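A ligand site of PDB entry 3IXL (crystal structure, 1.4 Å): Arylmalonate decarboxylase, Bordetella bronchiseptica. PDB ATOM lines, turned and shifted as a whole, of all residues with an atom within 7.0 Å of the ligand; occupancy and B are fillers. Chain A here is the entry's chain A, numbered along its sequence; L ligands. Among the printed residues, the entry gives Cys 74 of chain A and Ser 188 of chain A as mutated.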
ATOM      1  N   VAL A  13      10.347   8.314   3.305  1.00  0.00           N
ATOM      2  CA  VAL A  13      10.438   7.498   4.527  1.00  0.00           C
ATOM      3  C   VAL A  13       9.851   6.099   4.314  1.00  0.00           C
ATOM      4  O   VAL A  13       8.963   5.936   3.499  1.00  0.00           O
ATOM      5  CB  VAL A  13       9.741   8.211   5.725  1.00  0.00           C
ATOM      6  CG1 VAL A  13      10.394   9.571   6.013  1.00  0.00           C
ATOM      7  CG2 VAL A  13       8.235   8.389   5.494  1.00  0.00           C
ATOM      8  N   PRO A  14      10.387   5.084   5.011  1.00  0.00           N
ATOM      9  CA  PRO A  14       9.818   3.726   4.854  1.00  0.00           C
ATOM     10  C   PRO A  14       8.309   3.501   5.143  1.00  0.00           C
ATOM     11  O   PRO A  14       7.660   2.833   4.332  1.00  0.00           O
ATOM     12  CB  PRO A  14      10.716   2.858   5.738  1.00  0.00           C
ATOM     13  CG  PRO A  14      12.030   3.611   5.752  1.00  0.00           C
ATOM     14  CD  PRO A  14      11.618   5.058   5.825  1.00  0.00           C
ATOM     15  N   PRO A  15       7.744   4.029   6.251  1.00  0.00           N
ATOM     16  CA  PRO A  15       6.356   3.646   6.528  1.00  0.00           C
ATOM     17  C   PRO A  15       5.350   4.212   5.525  1.00  0.00           C
ATOM     18  O   PRO A  15       5.561   5.292   4.994  1.00  0.00           O
ATOM     19  CB  PRO A  15       6.104   4.221   7.929  1.00  0.00           C
ATOM     20  CG  PRO A  15       7.484   4.496   8.500  1.00  0.00           C
ATOM     21  CD  PRO A  15       8.270   4.920   7.303  1.00  0.00           C
ATOM     22  N   PRO A  21       9.935  11.869  10.269  1.00  0.00           N
ATOM     23  CA  PRO A  21      10.485  11.181  11.437  1.00  0.00           C
ATOM     24  C   PRO A  21      10.514  12.097  12.655  1.00  0.00           C
ATOM     25  O   PRO A  21      10.768  13.300  12.535  1.00  0.00           O
ATOM     26  CB  PRO A  21      11.899  10.776  10.974  1.00  0.00           C
ATOM     27  CG  PRO A  21      11.812  10.729   9.471  1.00  0.00           C
ATOM     28  CD  PRO A  21      10.830  11.815   9.105  1.00  0.00           C
ATOM     29  N   LEU A  40       7.259   0.360   3.042  1.00  0.00           N
ATOM     30  CA  LEU A  40       8.168  -0.775   3.224  1.00  0.00           C
ATOM     31  C   LEU A  40       7.548  -1.819   4.150  1.00  0.00           C
ATOM     32  O   LEU A  40       7.020  -1.467   5.205  1.00  0.00           O
ATOM     33  CB  LEU A  40       9.505  -0.286   3.803  1.00  0.00           C
ATOM     34  CG  LEU A  40      10.589  -1.326   4.100  1.00  0.00           C
ATOM     35  CD1 LEU A  40      11.097  -1.961   2.804  1.00  0.00           C
ATOM     36  CD2 LEU A  40      11.732  -0.694   4.868  1.00  0.00           C
ATOM     37  N   VAL A  43      12.312  -4.738   7.041  1.00  0.00           N
ATOM     38  CA  VAL A  43      13.659  -4.205   6.889  1.00  0.00           C
ATOM     39  C   VAL A  43      14.552  -5.383   6.484  1.00  0.00           C
ATOM     40  O   VAL A  43      15.341  -5.897   7.267  1.00  0.00           O
ATOM     41  CB  VAL A  43      14.122  -3.464   8.183  1.00  0.00           C
ATOM     42  CG1 VAL A  43      15.453  -2.789   7.975  1.00  0.00           C
ATOM     43  CG2 VAL A  43      13.045  -2.444   8.624  1.00  0.00           C
ATOM     44  N   TYR A  48      13.079  -4.381   0.662  1.00  0.00           N
ATOM     45  CA  TYR A  48      13.611  -3.271  -0.121  1.00  0.00           C
ATOM     46  C   TYR A  48      13.256  -3.405  -1.598  1.00  0.00           C
ATOM     47  O   TYR A  48      12.870  -2.432  -2.238  1.00  0.00           O
ATOM     48  CB  TYR A  48      15.133  -3.138   0.011  1.00  0.00           C
ATOM     49  CG  TYR A  48      15.661  -3.179   1.434  1.00  0.00           C
ATOM     50  CD1 TYR A  48      14.974  -2.548   2.482  1.00  0.00           C
ATOM     51  CD2 TYR A  48      16.846  -3.839   1.713  1.00  0.00           C
ATOM     52  CE1 TYR A  48      15.474  -2.610   3.793  1.00  0.00           C
ATOM     53  CE2 TYR A  48      17.342  -3.920   3.012  1.00  0.00           C
ATOM     54  CZ  TYR A  48      16.641  -3.309   4.038  1.00  0.00           C
ATOM     55  OH  TYR A  48      17.157  -3.397   5.316  1.00  0.00           O
ATOM     56  N   MET A  73      15.336   8.814   3.459  1.00  0.00           N
ATOM     57  CA  MET A  73      15.591   8.624   4.886  1.00  0.00           C
ATOM     58  C   MET A  73      15.495   7.155   5.319  1.00  0.00           C
ATOM     59  O   MET A  73      14.702   6.794   6.192  1.00  0.00           O
ATOM     60  CB  MET A  73      14.681   9.537   5.710  1.00  0.00           C
ATOM     61  CG  MET A  73      15.034  11.003   5.558  1.00  0.00           C
ATOM     62  SD  MET A  73      16.538  11.501   6.430  1.00  0.00           S
ATOM     63  CE  MET A  73      15.900  11.510   8.107  1.00  0.00           C
ATOM     64  N   CYS A  74      16.320   6.325   4.686  1.00  0.00           N
ATOM     65  CA  CYS A  74      16.478   4.928   5.079  1.00  0.00           C
ATOM     66  C   CYS A  74      17.900   4.518   4.756  1.00  0.00           C
ATOM     67  O   CYS A  74      18.361   4.668   3.627  1.00  0.00           O
ATOM     68  CB  CYS A  74      15.503   4.019   4.329  1.00  0.00           C
ATOM     69  SG  CYS A  74      15.677   2.273   4.817  1.00  0.00           S
ATOM     70  N   THR A  75      18.603   4.029   5.775  1.00  0.00           N
ATOM     71  CA  THR A  75      20.003   3.664   5.636  1.00  0.00           C
ATOM     72  C   THR A  75      20.094   2.402   4.779  1.00  0.00           C
ATOM     73  O   THR A  75      20.781   2.388   3.748  1.00  0.00           O
ATOM     74  CB  THR A  75      20.670   3.402   7.013  1.00  0.00           C
ATOM     75  OG1 THR A  75      20.005   4.143   8.053  1.00  0.00           O
ATOM     76  CG2 THR A  75      22.153   3.790   6.979  1.00  0.00           C
ATOM     77  N   SER A  76      19.392   1.358   5.193  1.00  0.00           N
ATOM     78  CA  SER A  76      19.543   0.071   4.531  1.00  0.00           C
ATOM     79  C   SER A  76      18.993   0.035   3.107  1.00  0.00           C
ATOM     80  O   SER A  76      19.570  -0.633   2.240  1.00  0.00           O
ATOM     81  CB  SER A  76      19.015  -1.068   5.411  1.00  0.00           C
ATOM     82  OG  SER A  76      17.655  -0.866   5.767  1.00  0.00           O
ATOM     83  N   LEU A  77      17.920   0.761   2.839  1.00  0.00           N
ATOM     84  CA  LEU A  77      17.393   0.861   1.474  1.00  0.00           C
ATOM     85  C   LEU A  77      18.447   1.460   0.558  1.00  0.00           C
ATOM     86  O   LEU A  77      18.494   1.139  -0.637  1.00  0.00           O
ATOM     87  CB  LEU A  77      16.142   1.729   1.462  1.00  0.00           C
ATOM     88  CG  LEU A  77      15.086   1.739   0.377  1.00  0.00           C
ATOM     89  CD1 LEU A  77      14.741   0.343  -0.100  1.00  0.00           C
ATOM     90  CD2 LEU A  77      13.878   2.338   1.036  1.00  0.00           C
ATOM     91  N   SER A  78      19.300   2.328   1.111  1.00  0.00           N
ATOM     92  CA  SER A  78      20.339   2.985   0.325  1.00  0.00           C
ATOM     93  C   SER A  78      21.717   2.294   0.317  1.00  0.00           C
ATOM     94  O   SER A  78      22.490   2.537  -0.602  1.00  0.00           O
ATOM     95  CB  SER A  78      20.451   4.475   0.664  1.00  0.00           C
ATOM     96  OG  SER A  78      20.657   4.719   2.056  1.00  0.00           O
ATOM     97  N   PHE A  79      21.986   1.406   1.276  1.00  0.00           N
ATOM     98  CA  PHE A  79      23.268   0.678   1.274  1.00  0.00           C
ATOM     99  C   PHE A  79      23.210  -0.796   0.852  1.00  0.00           C
ATOM    100  O   PHE A  79      24.278  -1.389   0.629  1.00  0.00           O
ATOM    101  CB  PHE A  79      24.077   0.856   2.595  1.00  0.00           C
ATOM    102  CG  PHE A  79      23.521   0.114   3.817  1.00  0.00           C
ATOM    103  CD1 PHE A  79      23.417  -1.283   3.839  1.00  0.00           C
ATOM    104  CD2 PHE A  79      23.156   0.833   4.949  1.00  0.00           C
ATOM    105  CE1 PHE A  79      22.913  -1.943   4.964  1.00  0.00           C
ATOM    106  CE2 PHE A  79      22.666   0.188   6.087  1.00  0.00           C
ATOM    107  CZ  PHE A  79      22.545  -1.200   6.094  1.00  0.00           C
ATOM    108  N   MET A 104      20.197   8.556   3.514  1.00  0.00           N
ATOM    109  CA  MET A 104      20.635   8.333   4.887  1.00  0.00           C
ATOM    110  C   MET A 104      21.987   7.612   4.956  1.00  0.00           C
ATOM    111  O   MET A 104      22.737   7.805   5.904  1.00  0.00           O
ATOM    112  CB  MET A 104      19.537   7.575   5.655  1.00  0.00           C
ATOM    113  CG  MET A 104      19.797   7.383   7.141  1.00  0.00           C
ATOM    114  SD  MET A 104      18.293   6.780   7.935  1.00  0.00           S
ATOM    115  CE  MET A 104      17.404   8.314   8.147  1.00  0.00           C
ATOM    116  N   TYR A 126      19.497  -4.418  12.971  1.00  0.00           N
ATOM    117  CA  TYR A 126      19.214  -5.351  11.865  1.00  0.00           C
ATOM    118  C   TYR A 126      19.535  -6.810  12.084  1.00  0.00           C
ATOM    119  O   TYR A 126      20.247  -7.186  13.014  1.00  0.00           O
ATOM    120  CB  TYR A 126      19.999  -4.944  10.620  1.00  0.00           C
ATOM    121  CG  TYR A 126      20.024  -3.487  10.246  1.00  0.00           C
ATOM    122  CD1 TYR A 126      21.244  -2.815  10.095  1.00  0.00           C
ATOM    123  CD2 TYR A 126      18.846  -2.801   9.975  1.00  0.00           C
ATOM    124  CE1 TYR A 126      21.277  -1.478   9.709  1.00  0.00           C
ATOM    125  CE2 TYR A 126      18.872  -1.449   9.591  1.00  0.00           C
ATOM    126  CZ  TYR A 126      20.102  -0.809   9.470  1.00  0.00           C
ATOM    127  OH  TYR A 126      20.163   0.514   9.077  1.00  0.00           O
ATOM    128  N   VAL A 130      21.667  -7.926   6.515  1.00  0.00           N
ATOM    129  CA  VAL A 130      21.720  -6.477   6.410  1.00  0.00           C
ATOM    130  C   VAL A 130      23.004  -5.929   7.075  1.00  0.00           C
ATOM    131  O   VAL A 130      23.651  -5.040   6.536  1.00  0.00           O
ATOM    132  CB  VAL A 130      20.442  -5.825   6.975  1.00  0.00           C
ATOM    133  CG1 VAL A 130      20.523  -4.303   6.905  1.00  0.00           C
ATOM    134  CG2 VAL A 130      19.219  -6.303   6.195  1.00  0.00           C
ATOM    135  N   GLY A 155      10.896  -5.583  11.731  1.00  0.00           N
ATOM    136  CA  GLY A 155       9.649  -4.811  11.705  1.00  0.00           C
ATOM    137  C   GLY A 155       9.907  -3.326  11.897  1.00  0.00           C
ATOM    138  O   GLY A 155      10.666  -2.943  12.781  1.00  0.00           O
ATOM    139  N   VAL A 156       9.275  -2.500  11.072  1.00  0.00           N
ATOM    140  CA  VAL A 156       9.416  -1.040  11.196  1.00  0.00           C
ATOM    141  C   VAL A 156       8.909  -0.529  12.551  1.00  0.00           C
ATOM    142  O   VAL A 156       9.633   0.186  13.260  1.00  0.00           O
ATOM    143  CB  VAL A 156       8.701  -0.308  10.028  1.00  0.00           C
ATOM    144  CG1 VAL A 156       8.623   1.191  10.297  1.00  0.00           C
ATOM    145  CG2 VAL A 156       9.412  -0.575   8.712  1.00  0.00           C
ATOM    146  N   GLU A 157       7.685  -0.898  12.922  1.00  0.00           N
ATOM    147  CA  GLU A 157       7.117  -0.507  14.224  1.00  0.00           C
ATOM    148  C   GLU A 157       7.910  -1.032  15.417  1.00  0.00           C
ATOM    149  O   GLU A 157       8.050  -0.332  16.438  1.00  0.00           O
ATOM    150  CB  GLU A 157       5.646  -0.940  14.329  1.00  0.00           C
ATOM    151  CG  GLU A 157       4.637   0.166  14.103  1.00  0.00           C
ATOM    152  CD  GLU A 157       4.931   1.008  12.880  1.00  0.00           C
ATOM    153  OE1 GLU A 157       4.957   0.455  11.751  1.00  0.00           O
ATOM    154  OE2 GLU A 157       5.154   2.222  13.045  1.00  0.00           O
ATOM    155  N   MET A 159      11.047  -1.413  15.686  1.00  0.00           N
ATOM    156  CA  MET A 159      12.242  -0.608  15.923  1.00  0.00           C
ATOM    157  C   MET A 159      11.940   0.641  16.758  1.00  0.00           C
ATOM    158  O   MET A 159      12.741   1.019  17.619  1.00  0.00           O
ATOM    159  CB  MET A 159      12.952  -0.261  14.614  1.00  0.00           C
ATOM    160  CG  MET A 159      13.848  -1.391  14.089  1.00  0.00           C
ATOM    161  SD  MET A 159      14.389  -1.005  12.448  1.00  0.00           S
ATOM    162  CE  MET A 159      14.961  -2.606  11.907  1.00  0.00           C
ATOM    163  N   SER A 187      22.935   2.251  13.721  1.00  0.00           N
ATOM    164  CA  SER A 187      22.274   2.194  12.422  1.00  0.00           C
ATOM    165  C   SER A 187      20.841   1.700  12.489  1.00  0.00           C
ATOM    166  O   SER A 187      20.552   0.651  13.067  1.00  0.00           O
ATOM    167  CB  SER A 187      23.091   1.372  11.415  1.00  0.00           C
ATOM    168  OG  SER A 187      22.647   1.628  10.093  1.00  0.00           O
ATOM    169  N   SER A 188      19.989   2.508  11.855  1.00  0.00           N
ATOM    170  CA  SER A 188      18.568   2.312  11.554  1.00  0.00           C
ATOM    171  C   SER A 188      17.827   3.573  11.922  1.00  0.00           C
ATOM    172  O   SER A 188      17.797   3.981  13.089  1.00  0.00           O
ATOM    173  CB  SER A 188      17.887   1.132  12.240  1.00  0.00           C
ATOM    174  OG  SER A 188      16.542   1.082  11.780  1.00  0.00           O
ATOM    175  N   GLY A 189      17.201   4.148  10.906  1.00  0.00           N
ATOM    176  CA  GLY A 189      16.398   5.350  11.059  1.00  0.00           C
ATOM    177  C   GLY A 189      15.071   5.070  11.722  1.00  0.00           C
ATOM    178  O   GLY A 189      14.266   5.980  11.892  1.00  0.00           O
ATOM    179  N   GLY A 190      14.834   3.816  12.090  1.00  0.00           N
ATOM    180  CA  GLY A 190      13.585   3.453  12.783  1.00  0.00           C
ATOM    181  C   GLY A 190      13.714   3.534  14.285  1.00  0.00           C
ATOM    182  O   GLY A 190      12.715   3.458  14.989  1.00  0.00           O
ATOM    183  N   LEU A 191      14.943   3.689  14.752  1.00  0.00           N
ATOM    184  CA  LEU A 191      15.237   3.778  16.179  1.00  0.00           C
ATOM    185  C   LEU A 191      15.086   5.201  16.683  1.00  0.00           C
ATOM    186  O   LEU A 191      15.391   6.157  15.960  1.00  0.00           O
ATOM    187  CB  LEU A 191      16.662   3.288  16.433  1.00  0.00           C
ATOM    188  CG  LEU A 191      16.968   1.828  16.076  1.00  0.00           C
ATOM    189  CD1 LEU A 191      18.451   1.570  16.181  1.00  0.00           C
ATOM    190  CD2 LEU A 191      16.170   0.876  16.953  1.00  0.00           C
ATOM    191  N   SER A 211      21.653   6.938  12.566  1.00  0.00           N
ATOM    192  CA  SER A 211      20.976   7.076  11.261  1.00  0.00           C
ATOM    193  C   SER A 211      19.977   8.247  11.148  1.00  0.00           C
ATOM    194  O   SER A 211      20.129   9.094  10.258  1.00  0.00           O
ATOM    195  CB  SER A 211      20.220   5.775  10.913  1.00  0.00           C
ATOM    196  OG  SER A 211      21.112   4.750  10.559  1.00  0.00           O
ATOM    197  N   SER A 212      18.951   8.261  11.988  1.00  0.00           N
ATOM    198  CA  SER A 212      17.914   9.286  11.834  1.00  0.00           C
ATOM    199  C   SER A 212      18.460  10.693  12.058  1.00  0.00           C
ATOM    200  O   SER A 212      18.323  11.562  11.202  1.00  0.00           O
ATOM    201  CB  SER A 212      16.706   8.973  12.714  1.00  0.00           C
ATOM    202  OG  SER A 212      15.649   9.862  12.444  1.00  0.00           O
HETATM  203  C1  LIG L   1      17.126   1.854   8.055  1.00  0.00           C
HETATM  204  C2  LIG L   1      15.717   1.315   8.180  1.00  0.00           C
HETATM  205  C3  LIG L   1      14.572   2.209   8.618  1.00  0.00           C
HETATM  206  C4  LIG L   1      13.516   1.563   9.272  1.00  0.00           C
HETATM  207  C5  LIG L   1      12.402   2.281   9.717  1.00  0.00           C
HETATM  208  C6  LIG L   1      12.340   3.659   9.488  1.00  0.00           C
HETATM  209  C7  LIG L   1      13.396   4.305   8.834  1.00  0.00           C
HETATM  210  C8  LIG L   1      14.510   3.587   8.390  1.00  0.00           C
HETATM  211  O1  LIG L   1      17.426   3.043   8.343  1.00  0.00           O
HETATM  212  O2  LIG L   1      17.985   1.021   7.640  1.00  0.00           O
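An oxygen (O2) of the ligand lies within hydrogen-bond range of the side-chain hydroxyl (OH) of Tyr 126.
N of Ser 76 sits at hydrogen-bond distance from O2 of the ligand (2.8 Å).
The side-chain hydroxyl (OG) of Ser 76 is in hydrogen-bond range of an oxygen (O2) of the ligand (2.7 Å).
The backbone NH of Gly 189 sits at hydrogen-bond distance from an oxygen (O1) of the ligand (2.8 Å).
N of Thr 75 is in hydrogen-bond range of O1 of the ligand, 3.0 Å away.
OG1 of Thr 75 sits at hydrogen-bond distance from O1 of the ligand (2.8 Å).
The side-chain hydroxyl (OH) of Tyr 126 lies within hydrogen-bond range of the side-chain hydroxyl (OG) of Ser 187, at 2.9 Å.
The side-chain hydroxyl (OG1) of Thr 75 sits at hydrogen-bond distance from the side-chain sulfur (SD) of Met 104 (3.1 Å).
The side-chain hydroxyl (OG) of Ser 211 is in hydrogen-bond range of the side-chain hydroxyl (OG1) of Thr 75, at 2.8 Å.
The side-chain hydroxyl (OG) of Ser 188 sits close to the backbone NH (N) of Gly 190 (3.2 Å).
OG of Ser 188 is in hydrogen-bond range of SD of Met 159 (3.1 Å).
N of Ser 188 sits at hydrogen-bond distance from OG of Ser 211, 2.8 Å away.
The side-chain sulfur of Cys 74 is in hydrogen-bond range of the backbone NH of Leu 77 (3.4 Å).
The side-chain hydroxyl (OG) of Ser 78 is in hydrogen-bond range of the backbone carbonyl oxygen (O) of Cys 74 (2.8 Å).
Merely in contact with the ligand: Pro 14 (3.4 Å), Met 73 (3.9 Å), Cys 74 (3.5 Å), Met 104 (3.9 Å), Val 156 (3.98 Å), Ser 188 (3.5 Å) and Gly 190 (3.5 Å).
Hydrophobic or aromatic side chains within 4 Å of the ligand: Pro 14, Met 104, Tyr 126 and Val 156.
11 residues have an atom within 4 Å of the ligand: Pro 14, Met 73, Cys 74, Thr 75, Ser 76, Met 104, Tyr 126, Val 156, Ser 188, Gly 189 and Gly 190.
The nearest printed residue that does not touch the ligand is Val 43 (4.1 Å).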
